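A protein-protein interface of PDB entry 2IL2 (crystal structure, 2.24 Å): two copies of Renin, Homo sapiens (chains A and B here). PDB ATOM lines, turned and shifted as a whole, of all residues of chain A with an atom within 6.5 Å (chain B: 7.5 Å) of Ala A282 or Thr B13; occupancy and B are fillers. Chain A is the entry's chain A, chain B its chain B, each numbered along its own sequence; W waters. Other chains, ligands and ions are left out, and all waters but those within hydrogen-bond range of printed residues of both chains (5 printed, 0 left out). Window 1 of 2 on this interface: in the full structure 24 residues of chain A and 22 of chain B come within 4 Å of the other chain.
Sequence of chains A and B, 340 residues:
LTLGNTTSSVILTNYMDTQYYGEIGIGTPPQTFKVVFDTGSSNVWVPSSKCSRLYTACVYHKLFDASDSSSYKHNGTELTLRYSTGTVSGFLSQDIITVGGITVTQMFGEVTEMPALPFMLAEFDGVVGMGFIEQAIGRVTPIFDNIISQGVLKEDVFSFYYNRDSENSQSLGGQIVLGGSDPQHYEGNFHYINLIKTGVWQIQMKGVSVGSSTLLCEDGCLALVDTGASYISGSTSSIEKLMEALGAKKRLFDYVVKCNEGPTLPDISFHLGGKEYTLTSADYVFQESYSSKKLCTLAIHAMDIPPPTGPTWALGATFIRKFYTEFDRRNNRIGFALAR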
ATOM      1  N   ARG A 164      -2.941   0.343 -12.401  1.00  0.00           N
ATOM      2  CA  ARG A 164      -2.736   0.184 -10.975  1.00  0.00           C
ATOM      3  C   ARG A 164      -1.999  -1.112 -10.694  1.00  0.00           C
ATOM      4  O   ARG A 164      -2.046  -2.055 -11.461  1.00  0.00           O
ATOM      5  CB  ARG A 164      -4.074   0.189 -10.253  1.00  0.00           C
ATOM      6  CG  ARG A 164      -4.757   1.558 -10.275  1.00  0.00           C
ATOM      7  CD  ARG A 164      -6.225   1.456 -10.639  1.00  0.00           C
ATOM      8  NE  ARG A 164      -7.024   2.586 -10.148  1.00  0.00           N
ATOM      9  CZ  ARG A 164      -7.280   3.712 -10.818  1.00  0.00           C
ATOM     10  NH1 ARG A 164      -8.031   4.650 -10.251  1.00  0.00           N
ATOM     11  NH2 ARG A 164      -6.797   3.928 -12.036  1.00  0.00           N
ATOM     12  N   GLY A 262      -5.589   9.017   5.590  1.00  0.00           N
ATOM     13  CA  GLY A 262      -5.449   8.922   4.139  1.00  0.00           C
ATOM     14  C   GLY A 262      -6.744   8.942   3.331  1.00  0.00           C
ATOM     15  O   GLY A 262      -6.890   9.760   2.422  1.00  0.00           O
ATOM     16  N   PRO A 263      -7.698   8.043   3.652  1.00  0.00           N
ATOM     17  CA  PRO A 263      -8.864   7.868   2.786  1.00  0.00           C
ATOM     18  C   PRO A 263      -9.755   9.090   2.693  1.00  0.00           C
ATOM     19  O   PRO A 263     -10.505   9.225   1.719  1.00  0.00           O
ATOM     20  CB  PRO A 263      -9.623   6.716   3.451  1.00  0.00           C
ATOM     21  CG  PRO A 263      -8.641   6.037   4.288  1.00  0.00           C
ATOM     22  CD  PRO A 263      -7.751   7.112   4.791  1.00  0.00           C
ATOM     23  N   LEU A 265      -8.618  12.380   2.869  1.00  0.00           N
ATOM     24  CA  LEU A 265      -7.942  13.558   2.330  1.00  0.00           C
ATOM     25  C   LEU A 265      -8.701  14.089   1.093  1.00  0.00           C
ATOM     26  O   LEU A 265      -9.395  13.334   0.396  1.00  0.00           O
ATOM     27  CB  LEU A 265      -6.493  13.247   1.956  1.00  0.00           C
ATOM     28  CG  LEU A 265      -5.498  12.777   3.030  1.00  0.00           C
ATOM     29  CD1 LEU A 265      -4.092  12.618   2.409  1.00  0.00           C
ATOM     30  CD2 LEU A 265      -5.468  13.735   4.223  1.00  0.00           C
ATOM     31  N   LEU A 279      -7.875  14.029  -9.034  1.00  0.00           N
ATOM     32  CA  LEU A 279      -7.449  12.862  -8.278  1.00  0.00           C
ATOM     33  C   LEU A 279      -8.113  12.842  -6.889  1.00  0.00           C
ATOM     34  O   LEU A 279      -8.140  13.843  -6.190  1.00  0.00           O
ATOM     35  CB  LEU A 279      -5.927  12.855  -8.125  1.00  0.00           C
ATOM     36  CG  LEU A 279      -4.997  12.894  -9.359  1.00  0.00           C
ATOM     37  CD1 LEU A 279      -3.600  12.325  -9.004  1.00  0.00           C
ATOM     38  CD2 LEU A 279      -5.564  12.163 -10.543  1.00  0.00           C
ATOM     39  N   THR A 280      -8.647  11.692  -6.502  1.00  0.00           N
ATOM     40  CA  THR A 280      -9.066  11.468  -5.122  1.00  0.00           C
ATOM     41  C   THR A 280      -7.877  10.952  -4.299  1.00  0.00           C
ATOM     42  O   THR A 280      -6.839  10.602  -4.850  1.00  0.00           O
ATOM     43  CB  THR A 280     -10.192  10.444  -5.045  1.00  0.00           C
ATOM     44  OG1 THR A 280      -9.675   9.151  -5.375  1.00  0.00           O
ATOM     45  CG2 THR A 280     -11.327  10.824  -6.007  1.00  0.00           C
ATOM     46  N   SER A 281      -8.049  10.873  -2.984  1.00  0.00           N
ATOM     47  CA  SER A 281      -6.991  10.393  -2.101  1.00  0.00           C
ATOM     48  C   SER A 281      -6.549   8.953  -2.419  1.00  0.00           C
ATOM     49  O   SER A 281      -5.374   8.634  -2.289  1.00  0.00           O
ATOM     50  CB  SER A 281      -7.398  10.531  -0.645  1.00  0.00           C
ATOM     51  OG  SER A 281      -8.550   9.766  -0.371  1.00  0.00           O
ATOM     52  N   ALA A 282      -7.494   8.120  -2.858  1.00  0.00           N
ATOM     53  CA  ALA A 282      -7.207   6.771  -3.338  1.00  0.00           C
ATOM     54  C   ALA A 282      -6.200   6.760  -4.498  1.00  0.00           C
ATOM     55  O   ALA A 282      -5.476   5.793  -4.666  1.00  0.00           O
ATOM     56  CB  ALA A 282      -8.498   6.078  -3.756  1.00  0.00           C
ATOM     57  N   ASP A 283      -6.194   7.814  -5.304  1.00  0.00           N
ATOM     58  CA  ASP A 283      -5.266   7.975  -6.418  1.00  0.00           C
ATOM     59  C   ASP A 283      -3.853   8.452  -6.040  1.00  0.00           C
ATOM     60  O   ASP A 283      -2.908   8.160  -6.774  1.00  0.00           O
ATOM     61  CB  ASP A 283      -5.855   8.957  -7.456  1.00  0.00           C
ATOM     62  CG  ASP A 283      -7.195   8.505  -7.991  1.00  0.00           C
ATOM     63  OD1 ASP A 283      -7.295   7.314  -8.363  1.00  0.00           O
ATOM     64  OD2 ASP A 283      -8.164   9.317  -8.019  1.00  0.00           O
ATOM     65  N   TYR A 284      -3.692   9.205  -4.944  1.00  0.00           N
ATOM     66  CA  TYR A 284      -2.367   9.729  -4.573  1.00  0.00           C
ATOM     67  C   TYR A 284      -1.811   9.332  -3.199  1.00  0.00           C
ATOM     68  O   TYR A 284      -0.715   9.763  -2.828  1.00  0.00           O
ATOM     69  CB  TYR A 284      -2.346  11.247  -4.723  1.00  0.00           C
ATOM     70  CG  TYR A 284      -3.193  12.008  -3.738  1.00  0.00           C
ATOM     71  CD1 TYR A 284      -2.683  12.378  -2.511  1.00  0.00           C
ATOM     72  CD2 TYR A 284      -4.497  12.405  -4.060  1.00  0.00           C
ATOM     73  CE1 TYR A 284      -3.432  13.105  -1.613  1.00  0.00           C
ATOM     74  CE2 TYR A 284      -5.272  13.141  -3.163  1.00  0.00           C
ATOM     75  CZ  TYR A 284      -4.728  13.492  -1.935  1.00  0.00           C
ATOM     76  OH  TYR A 284      -5.450  14.216  -1.013  1.00  0.00           O
ATOM     77  N   VAL A 285      -2.552   8.517  -2.453  1.00  0.00           N
ATOM     78  CA  VAL A 285      -2.063   7.965  -1.188  1.00  0.00           C
ATOM     79  C   VAL A 285      -1.717   6.495  -1.386  1.00  0.00           C
ATOM     80  O   VAL A 285      -2.492   5.738  -1.976  1.00  0.00           O
ATOM     81  CB  VAL A 285      -3.127   8.089  -0.054  1.00  0.00           C
ATOM     82  CG1 VAL A 285      -2.584   7.519   1.289  1.00  0.00           C
ATOM     83  CG2 VAL A 285      -3.541   9.528   0.111  1.00  0.00           C
ATOM     84  N   PHE A 286      -0.554   6.086  -0.889  1.00  0.00           N
ATOM     85  CA  PHE A 286      -0.239   4.663  -0.815  1.00  0.00           C
ATOM     86  C   PHE A 286      -0.844   4.153   0.474  1.00  0.00           C
ATOM     87  O   PHE A 286      -0.207   4.200   1.522  1.00  0.00           O
ATOM     88  CB  PHE A 286       1.259   4.424  -0.792  1.00  0.00           C
ATOM     89  CG  PHE A 286       1.921   4.578  -2.119  1.00  0.00           C
ATOM     90  CD1 PHE A 286       2.500   5.789  -2.481  1.00  0.00           C
ATOM     91  CD2 PHE A 286       1.997   3.507  -2.990  1.00  0.00           C
ATOM     92  CE1 PHE A 286       3.127   5.932  -3.680  1.00  0.00           C
ATOM     93  CE2 PHE A 286       2.629   3.643  -4.213  1.00  0.00           C
ATOM     94  CZ  PHE A 286       3.195   4.856  -4.560  1.00  0.00           C
ATOM     95  N   GLN A 287      -2.088   3.699   0.383  1.00  0.00           N
ATOM     96  CA  GLN A 287      -2.841   3.223   1.528  1.00  0.00           C
ATOM     97  C   GLN A 287      -2.396   1.811   1.877  1.00  0.00           C
ATOM     98  O   GLN A 287      -2.756   0.859   1.197  1.00  0.00           O
ATOM     99  CB  GLN A 287      -4.339   3.249   1.202  1.00  0.00           C
ATOM    100  CG  GLN A 287      -5.226   3.266   2.410  1.00  0.00           C
ATOM    101  CD  GLN A 287      -5.076   4.547   3.216  1.00  0.00           C
ATOM    102  OE1 GLN A 287      -5.179   5.645   2.673  1.00  0.00           O
ATOM    103  NE2 GLN A 287      -4.837   4.407   4.513  1.00  0.00           N
ATOM    104  N   VAL B  10     -16.275   2.113 -14.283  1.00  0.00           N
ATOM    105  CA  VAL B  10     -15.923   3.008 -13.195  1.00  0.00           C
ATOM    106  C   VAL B  10     -15.155   2.201 -12.156  1.00  0.00           C
ATOM    107  O   VAL B  10     -15.656   1.214 -11.621  1.00  0.00           O
ATOM    108  CB  VAL B  10     -17.168   3.682 -12.585  1.00  0.00           C
ATOM    109  CG1 VAL B  10     -16.766   4.553 -11.384  1.00  0.00           C
ATOM    110  CG2 VAL B  10     -17.894   4.504 -13.653  1.00  0.00           C
ATOM    111  N   ILE B  11     -13.929   2.624 -11.914  1.00  0.00           N
ATOM    112  CA  ILE B  11     -13.051   2.067 -10.905  1.00  0.00           C
ATOM    113  C   ILE B  11     -13.495   2.479  -9.489  1.00  0.00           C
ATOM    114  O   ILE B  11     -13.817   3.655  -9.229  1.00  0.00           O
ATOM    115  CB  ILE B  11     -11.592   2.493 -11.217  1.00  0.00           C
ATOM    116  CG1 ILE B  11     -11.146   1.771 -12.492  1.00  0.00           C
ATOM    117  CG2 ILE B  11     -10.647   2.230 -10.031  1.00  0.00           C
ATOM    118  CD1 ILE B  11      -9.828   2.257 -13.089  1.00  0.00           C
ATOM    119  N   LEU B  12     -13.514   1.493  -8.588  1.00  0.00           N
ATOM    120  CA  LEU B  12     -14.067   1.664  -7.254  1.00  0.00           C
ATOM    121  C   LEU B  12     -12.948   1.608  -6.240  1.00  0.00           C
ATOM    122  O   LEU B  12     -11.945   0.914  -6.430  1.00  0.00           O
ATOM    123  CB  LEU B  12     -15.142   0.604  -6.932  1.00  0.00           C
ATOM    124  CG  LEU B  12     -16.358   0.458  -7.867  1.00  0.00           C
ATOM    125  CD1 LEU B  12     -17.303  -0.622  -7.342  1.00  0.00           C
ATOM    126  CD2 LEU B  12     -17.111   1.755  -8.100  1.00  0.00           C
ATOM    127  N   THR B  13     -13.100   2.396  -5.180  1.00  0.00           N
ATOM    128  CA  THR B  13     -12.204   2.316  -4.027  1.00  0.00           C
ATOM    129  C   THR B  13     -12.837   1.343  -3.028  1.00  0.00           C
ATOM    130  O   THR B  13     -14.041   1.387  -2.775  1.00  0.00           O
ATOM    131  CB  THR B  13     -11.999   3.691  -3.373  1.00  0.00           C
ATOM    132  OG1 THR B  13     -11.362   4.569  -4.304  1.00  0.00           O
ATOM    133  CG2 THR B  13     -11.149   3.587  -2.120  1.00  0.00           C
ATOM    134  N   ASN B  14     -12.004   0.467  -2.487  1.00  0.00           N
ATOM    135  CA  ASN B  14     -12.358  -0.461  -1.419  1.00  0.00           C
ATOM    136  C   ASN B  14     -11.855   0.138  -0.122  1.00  0.00           C
ATOM    137  O   ASN B  14     -10.647   0.293   0.068  1.00  0.00           O
ATOM    138  CB  ASN B  14     -11.687  -1.810  -1.660  1.00  0.00           C
ATOM    139  CG  ASN B  14     -12.035  -2.846  -0.614  1.00  0.00           C
ATOM    140  OD1 ASN B  14     -12.578  -2.537   0.444  1.00  0.00           O
ATOM    141  ND2 ASN B  14     -11.700  -4.096  -0.903  1.00  0.00           N
ATOM    142  N   TYR B  15     -12.791   0.498   0.753  1.00  0.00           N
ATOM    143  CA  TYR B  15     -12.473   0.872   2.105  1.00  0.00           C
ATOM    144  C   TYR B  15     -12.791  -0.265   3.083  1.00  0.00           C
ATOM    145  O   TYR B  15     -13.949  -0.546   3.349  1.00  0.00           O
ATOM    146  CB  TYR B  15     -13.246   2.124   2.495  1.00  0.00           C
ATOM    147  CG  TYR B  15     -12.947   2.583   3.914  1.00  0.00           C
ATOM    148  CD1 TYR B  15     -11.740   3.181   4.222  1.00  0.00           C
ATOM    149  CD2 TYR B  15     -13.877   2.429   4.920  1.00  0.00           C
ATOM    150  CE1 TYR B  15     -11.459   3.611   5.528  1.00  0.00           C
ATOM    151  CE2 TYR B  15     -13.619   2.858   6.218  1.00  0.00           C
ATOM    152  CZ  TYR B  15     -12.406   3.438   6.520  1.00  0.00           C
ATOM    153  OH  TYR B  15     -12.155   3.860   7.797  1.00  0.00           O
ATOM    154  N   MET B  16     -11.742  -0.893   3.609  1.00  0.00           N
ATOM    155  CA  MET B  16     -11.826  -1.916   4.656  1.00  0.00           C
ATOM    156  C   MET B  16     -12.731  -3.122   4.363  1.00  0.00           C
ATOM    157  O   MET B  16     -13.260  -3.737   5.282  1.00  0.00           O
ATOM    158  CB  MET B  16     -12.259  -1.264   5.965  1.00  0.00           C
ATOM    159  CG  MET B  16     -11.218  -0.372   6.558  1.00  0.00           C
ATOM    160  SD  MET B  16     -11.811   0.319   8.100  1.00  0.00           S
ATOM    161  CE  MET B  16     -12.065  -1.217   9.025  1.00  0.00           C
ATOM    162  N   GLN B  19     -16.959  -0.701   2.461  1.00  0.00           N
ATOM    163  CA  GLN B  19     -17.498   0.335   1.590  1.00  0.00           C
ATOM    164  C   GLN B  19     -16.770   0.271   0.260  1.00  0.00           C
ATOM    165  O   GLN B  19     -15.536   0.104   0.226  1.00  0.00           O
ATOM    166  CB  GLN B  19     -17.342   1.736   2.188  1.00  0.00           C
ATOM    167  CG  GLN B  19     -17.689   1.840   3.656  1.00  0.00           C
ATOM    168  CD  GLN B  19     -17.605   3.245   4.193  1.00  0.00           C
ATOM    169  OE1 GLN B  19     -17.710   4.221   3.447  1.00  0.00           O
ATOM    170  NE2 GLN B  19     -17.410   3.362   5.504  1.00  0.00           N
ATOM    171  N   TYR B  20     -17.543   0.391  -0.815  1.00  0.00           N
ATOM    172  CA  TYR B  20     -17.040   0.410  -2.164  1.00  0.00           C
ATOM    173  C   TYR B  20     -17.683   1.556  -2.929  1.00  0.00           C
ATOM    174  O   TYR B  20     -18.902   1.590  -3.072  1.00  0.00           O
ATOM    175  CB  TYR B  20     -17.381  -0.919  -2.857  1.00  0.00           C
ATOM    176  CG  TYR B  20     -16.614  -2.135  -2.332  1.00  0.00           C
ATOM    177  CD1 TYR B  20     -17.074  -2.865  -1.244  1.00  0.00           C
ATOM    178  CD2 TYR B  20     -15.440  -2.545  -2.927  1.00  0.00           C
ATOM    179  CE1 TYR B  20     -16.393  -3.986  -0.790  1.00  0.00           C
ATOM    180  CE2 TYR B  20     -14.746  -3.657  -2.461  1.00  0.00           C
ATOM    181  CZ  TYR B  20     -15.244  -4.381  -1.407  1.00  0.00           C
ATOM    182  OH  TYR B  20     -14.530  -5.487  -0.946  1.00  0.00           O
ATOM    183  N   TYR B  21     -16.869   2.476  -3.445  1.00  0.00           N
ATOM    184  CA  TYR B  21     -17.378   3.685  -4.098  1.00  0.00           C
ATOM    185  C   TYR B  21     -16.459   4.180  -5.213  1.00  0.00           C
ATOM    186  O   TYR B  21     -15.254   3.924  -5.210  1.00  0.00           O
ATOM    187  CB  TYR B  21     -17.570   4.801  -3.061  1.00  0.00           C
ATOM    188  CG  TYR B  21     -16.409   4.916  -2.086  1.00  0.00           C
ATOM    189  CD1 TYR B  21     -16.380   4.146  -0.929  1.00  0.00           C
ATOM    190  CD2 TYR B  21     -15.336   5.765  -2.336  1.00  0.00           C
ATOM    191  CE1 TYR B  21     -15.332   4.224  -0.030  1.00  0.00           C
ATOM    192  CE2 TYR B  21     -14.266   5.855  -1.436  1.00  0.00           C
ATOM    193  CZ  TYR B  21     -14.274   5.064  -0.283  1.00  0.00           C
ATOM    194  OH  TYR B  21     -13.224   5.096   0.618  1.00  0.00           O
ATOM    195  N   GLY B  22     -17.034   4.919  -6.157  1.00  0.00           N
ATOM    196  CA  GLY B  22     -16.285   5.455  -7.286  1.00  0.00           C
ATOM    197  C   GLY B  22     -16.766   6.842  -7.604  1.00  0.00           C
ATOM    198  O   GLY B  22     -17.690   7.326  -6.973  1.00  0.00           O
ATOM    199  N   GLU B  23     -16.131   7.473  -8.597  1.00  0.00           N
ATOM    200  CA  GLU B  23     -16.410   8.860  -8.966  1.00  0.00           C
ATOM    201  C   GLU B  23     -17.570   8.999  -9.951  1.00  0.00           C
ATOM    202  O   GLU B  23     -17.690   8.252 -10.915  1.00  0.00           O
ATOM    203  CB  GLU B  23     -15.167   9.520  -9.582  1.00  0.00           C
ATOM    204  CG  GLU B  23     -13.907   9.483  -8.709  1.00  0.00           C
ATOM    205  CD  GLU B  23     -12.646  10.031  -9.411  1.00  0.00           C
ATOM    206  OE1 GLU B  23     -12.727  11.101 -10.062  1.00  0.00           O
ATOM    207  OE2 GLU B  23     -11.561   9.398  -9.287  1.00  0.00           O
ATOM    208  N   LYS B  34     -17.796  11.016  -4.563  1.00  0.00           N
ATOM    209  CA  LYS B  34     -17.609   9.591  -4.307  1.00  0.00           C
ATOM    210  C   LYS B  34     -18.961   8.949  -4.052  1.00  0.00           C
ATOM    211  O   LYS B  34     -19.665   9.369  -3.145  1.00  0.00           O
ATOM    212  CB  LYS B  34     -16.695   9.408  -3.096  1.00  0.00           C
ATOM    213  CG  LYS B  34     -15.269   9.836  -3.378  1.00  0.00           C
ATOM    214  CD  LYS B  34     -14.411   9.793  -2.125  1.00  0.00           C
ATOM    215  CE  LYS B  34     -13.026  10.391  -2.385  1.00  0.00           C
ATOM    216  NZ  LYS B  34     -12.387  10.796  -1.112  1.00  0.00           N
ATOM    217  N   VAL B  35     -19.349   7.947  -4.845  1.00  0.00           N
ATOM    218  CA  VAL B  35     -20.681   7.340  -4.655  1.00  0.00           C
ATOM    219  C   VAL B  35     -20.639   5.830  -4.558  1.00  0.00           C
ATOM    220  O   VAL B  35     -19.821   5.183  -5.199  1.00  0.00           O
ATOM    221  CB  VAL B  35     -21.713   7.733  -5.761  1.00  0.00           C
ATOM    222  CG1 VAL B  35     -22.047   9.193  -5.689  1.00  0.00           C
ATOM    223  CG2 VAL B  35     -21.219   7.350  -7.155  1.00  0.00           C
ATOM    224  N   GLU B 123     -17.307   6.997   3.811  1.00  0.00           N
ATOM    225  CA  GLU B 123     -16.168   7.526   3.071  1.00  0.00           C
ATOM    226  C   GLU B 123     -16.631   8.061   1.736  1.00  0.00           C
ATOM    227  O   GLU B 123     -15.899   8.770   1.055  1.00  0.00           O
ATOM    228  CB  GLU B 123     -15.121   6.442   2.835  1.00  0.00           C
ATOM    229  CG  GLU B 123     -14.364   5.995   4.062  1.00  0.00           C
ATOM    230  CD  GLU B 123     -13.475   7.075   4.606  1.00  0.00           C
ATOM    231  OE1 GLU B 123     -13.091   7.982   3.822  1.00  0.00           O
ATOM    232  OE2 GLU B 123     -13.174   7.025   5.817  1.00  0.00           O
ATOM    233  N   TYR B 162     -16.042  -6.587  -6.987  1.00  0.00           N
ATOM    234  CA  TYR B 162     -15.558  -6.072  -5.699  1.00  0.00           C
ATOM    235  C   TYR B 162     -14.334  -6.872  -5.292  1.00  0.00           C
ATOM    236  O   TYR B 162     -14.383  -8.100  -5.165  1.00  0.00           O
ATOM    237  CB  TYR B 162     -16.620  -6.215  -4.591  1.00  0.00           C
ATOM    238  CG  TYR B 162     -17.735  -5.188  -4.541  1.00  0.00           C
ATOM    239  CD1 TYR B 162     -18.792  -5.319  -3.626  1.00  0.00           C
ATOM    240  CD2 TYR B 162     -17.768  -4.098  -5.400  1.00  0.00           C
ATOM    241  CE1 TYR B 162     -19.821  -4.378  -3.558  1.00  0.00           C
ATOM    242  CE2 TYR B 162     -18.784  -3.156  -5.331  1.00  0.00           C
ATOM    243  CZ  TYR B 162     -19.809  -3.293  -4.417  1.00  0.00           C
ATOM    244  OH  TYR B 162     -20.800  -2.319  -4.394  1.00  0.00           O
ATOM    245  N   GLN B 170      -1.533  -1.453  -4.134  1.00  0.00           N
ATOM    246  CA  GLN B 170      -2.463  -0.363  -4.472  1.00  0.00           C
ATOM    247  C   GLN B 170      -3.350  -0.800  -5.649  1.00  0.00           C
ATOM    248  O   GLN B 170      -3.507  -0.085  -6.634  1.00  0.00           O
ATOM    249  CB  GLN B 170      -1.709   0.933  -4.789  1.00  0.00           C
ATOM    250  CG  GLN B 170      -0.810   1.425  -3.653  1.00  0.00           C
ATOM    251  CD  GLN B 170      -1.556   1.497  -2.325  1.00  0.00           C
ATOM    252  OE1 GLN B 170      -1.076   0.990  -1.295  1.00  0.00           O
ATOM    253  NE2 GLN B 170      -2.745   2.103  -2.349  1.00  0.00           N
ATOM    254  N   SER B 171      -3.935  -1.989  -5.514  1.00  0.00           N
ATOM    255  CA  SER B 171      -4.709  -2.631  -6.587  1.00  0.00           C
ATOM    256  C   SER B 171      -6.124  -2.071  -6.658  1.00  0.00           C
ATOM    257  O   SER B 171      -6.556  -1.398  -5.730  1.00  0.00           O
ATOM    258  CB  SER B 171      -4.748  -4.145  -6.342  1.00  0.00           C
ATOM    259  OG  SER B 171      -5.218  -4.406  -5.037  1.00  0.00           O
ATOM    260  N   LEU B 172      -6.861  -2.338  -7.741  1.00  0.00           N
ATOM    261  CA  LEU B 172      -8.185  -1.738  -7.844  1.00  0.00           C
ATOM    262  C   LEU B 172      -9.072  -2.276  -6.718  1.00  0.00           C
ATOM    263  O   LEU B 172      -8.980  -3.443  -6.339  1.00  0.00           O
ATOM    264  CB  LEU B 172      -8.813  -1.883  -9.244  1.00  0.00           C
ATOM    265  CG  LEU B 172      -9.465  -3.178  -9.718  1.00  0.00           C
ATOM    266  CD1 LEU B 172     -10.107  -2.978 -11.061  1.00  0.00           C
ATOM    267  CD2 LEU B 172      -8.443  -4.302  -9.789  1.00  0.00           C
ATOM    268  N   GLY B 173      -9.894  -1.400  -6.158  1.00  0.00           N
ATOM    269  CA  GLY B 173     -10.848  -1.785  -5.119  1.00  0.00           C
ATOM    270  C   GLY B 173     -12.051  -2.509  -5.685  1.00  0.00           C
ATOM    271  O   GLY B 173     -12.674  -3.301  -5.005  1.00  0.00           O
ATOM    272  N   GLY B 174     -12.381  -2.194  -6.937  1.00  0.00           N
ATOM    273  CA  GLY B 174     -13.498  -2.820  -7.646  1.00  0.00           C
ATOM    274  C   GLY B 174     -13.724  -2.118  -8.975  1.00  0.00           C
ATOM    275  O   GLY B 174     -13.000  -1.179  -9.338  1.00  0.00           O
ATOM    276  N   GLN B 175     -14.739  -2.581  -9.698  1.00  0.00           N
ATOM    277  CA  GLN B 175     -15.098  -2.003 -10.975  1.00  0.00           C
ATOM    278  C   GLN B 175     -16.577  -2.277 -11.260  1.00  0.00           C
ATOM    279  O   GLN B 175     -17.062  -3.395 -11.071  1.00  0.00           O
ATOM    280  CB  GLN B 175     -14.201  -2.596 -12.060  1.00  0.00           C
ATOM    281  CG  GLN B 175     -14.374  -2.047 -13.447  1.00  0.00           C
ATOM    282  CD  GLN B 175     -13.908  -3.030 -14.482  1.00  0.00           C
ATOM    283  OE1 GLN B 175     -12.971  -2.767 -15.240  1.00  0.00           O
ATOM    284  NE2 GLN B 175     -14.522  -4.202 -14.485  1.00  0.00           N
HETATM  285  O   HOH W   1     -11.203   6.865   0.031  1.00  0.00           O
HETATM  286  O   HOH W   2     -11.893   7.349  -4.092  1.00  0.00           O
HETATM  287  O   HOH W   3     -10.504  12.570  -1.902  1.00  0.00           O
HETATM  288  O   HOH W   4     -13.187   9.173   0.946  1.00  0.00           O
HETATM  289  O   HOH W   5     -12.205  12.759   0.735  1.00  0.00           O
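The backbone carbonyl oxygen (O) of Gln A287 lies close to the side-chain amide oxygen (OE1) of Gln B170, 3.0 Å away.
The side-chain carboxylate (OD1) of Asp A283 is in salt-bridge range of the guanidinium group (NH1) of Arg A164, 3.3 Å away. OG of Ser A281 is in hydrogen-bond range of O of Pro A263 (2.9 Å). The side-chain hydroxyl of Thr A280 lies close to the backbone NH of Ala A282. OD2 of Asp A283 sits at hydrogen-bond distance from N of Thr A280 (2.9 Å). The backbone carbonyl oxygen (O) of Tyr B21 is in hydrogen-bond range of the backbone NH (N) of Thr B13 (2.6 Å). SD of Met B16 lies close to OH of Tyr B15, at 3.6 Å.
Among the printed residues, pairs that only touch across the chains: Arg A164 with Ile B11, Arg A164 with Gln B170, Pro A263 with Tyr B15, Pro A263 with Lys B34, Pro A263 with Glu B123, Thr A280 with Glu B23, Thr A280 with Lys B34, Ala A282 with Thr B13, Asp A283 with Glu B23, Val A285 with Gln B170 and Phe A286 with Gln B170.
Thr B13 touches just one residue of chain A: Ala A282. No residue of chain B comes within 4 Å of Ser A281. Printed residues of chain A within 4 Å of Glu B23: Thr A280 and Asp A283. Of the printed residues of chain B, Gln A287 touches Gln B170 (3.0 Å). Gly B22 touches none of the printed residues of chain A. Gln B19 touches none of the printed residues of chain A. The nearest residue of chain A that does not touch Thr B13 is Thr A280 (5.0 Å).
Printed residues of chain B that touch a printed residue of chain A: Ile B11, Thr B13, Tyr B15, Glu B23, Lys B34, Glu B123 and Gln B170. Hydrophobic or aromatic side chains of chain A within 4 Å of the printed part of chain B: Pro A263, Ala A282 and Phe A286. Among the printed residues, no Asp or Glu carboxylate lies within 4 Å of a Lys or Arg side-chain nitrogen of the other chain.
No position is printed for both chains. Of the 12 pairs that touch across the chains among the printed residues, none has its exchanged pair printed and touching as well.
Water W3 lies within hydrogen-bond range of O of Leu A265, NZ of Lys B34 and N of Ser A281. Water W5 lies within hydrogen-bond range of NZ of Lys B34 (2.7 Å) and O of Leu A265 (2.9 Å). Water W4 lies within hydrogen-bond range of the side-chain amino group of Lys B34, the backbone carbonyl oxygen of Glu B123 and the backbone carbonyl oxygen of Pro A263. Water W1 lies within hydrogen-bond range of the side-chain hydroxyl (OH) of Tyr B21 (2.7 Å) and the backbone carbonyl oxygen (O) of Pro A263 (3.0 Å). Water W2 bridges the side-chain hydroxyl of Thr B13 (2.8 Å) and the side-chain hydroxyl of Thr A280 (3.1 Å).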
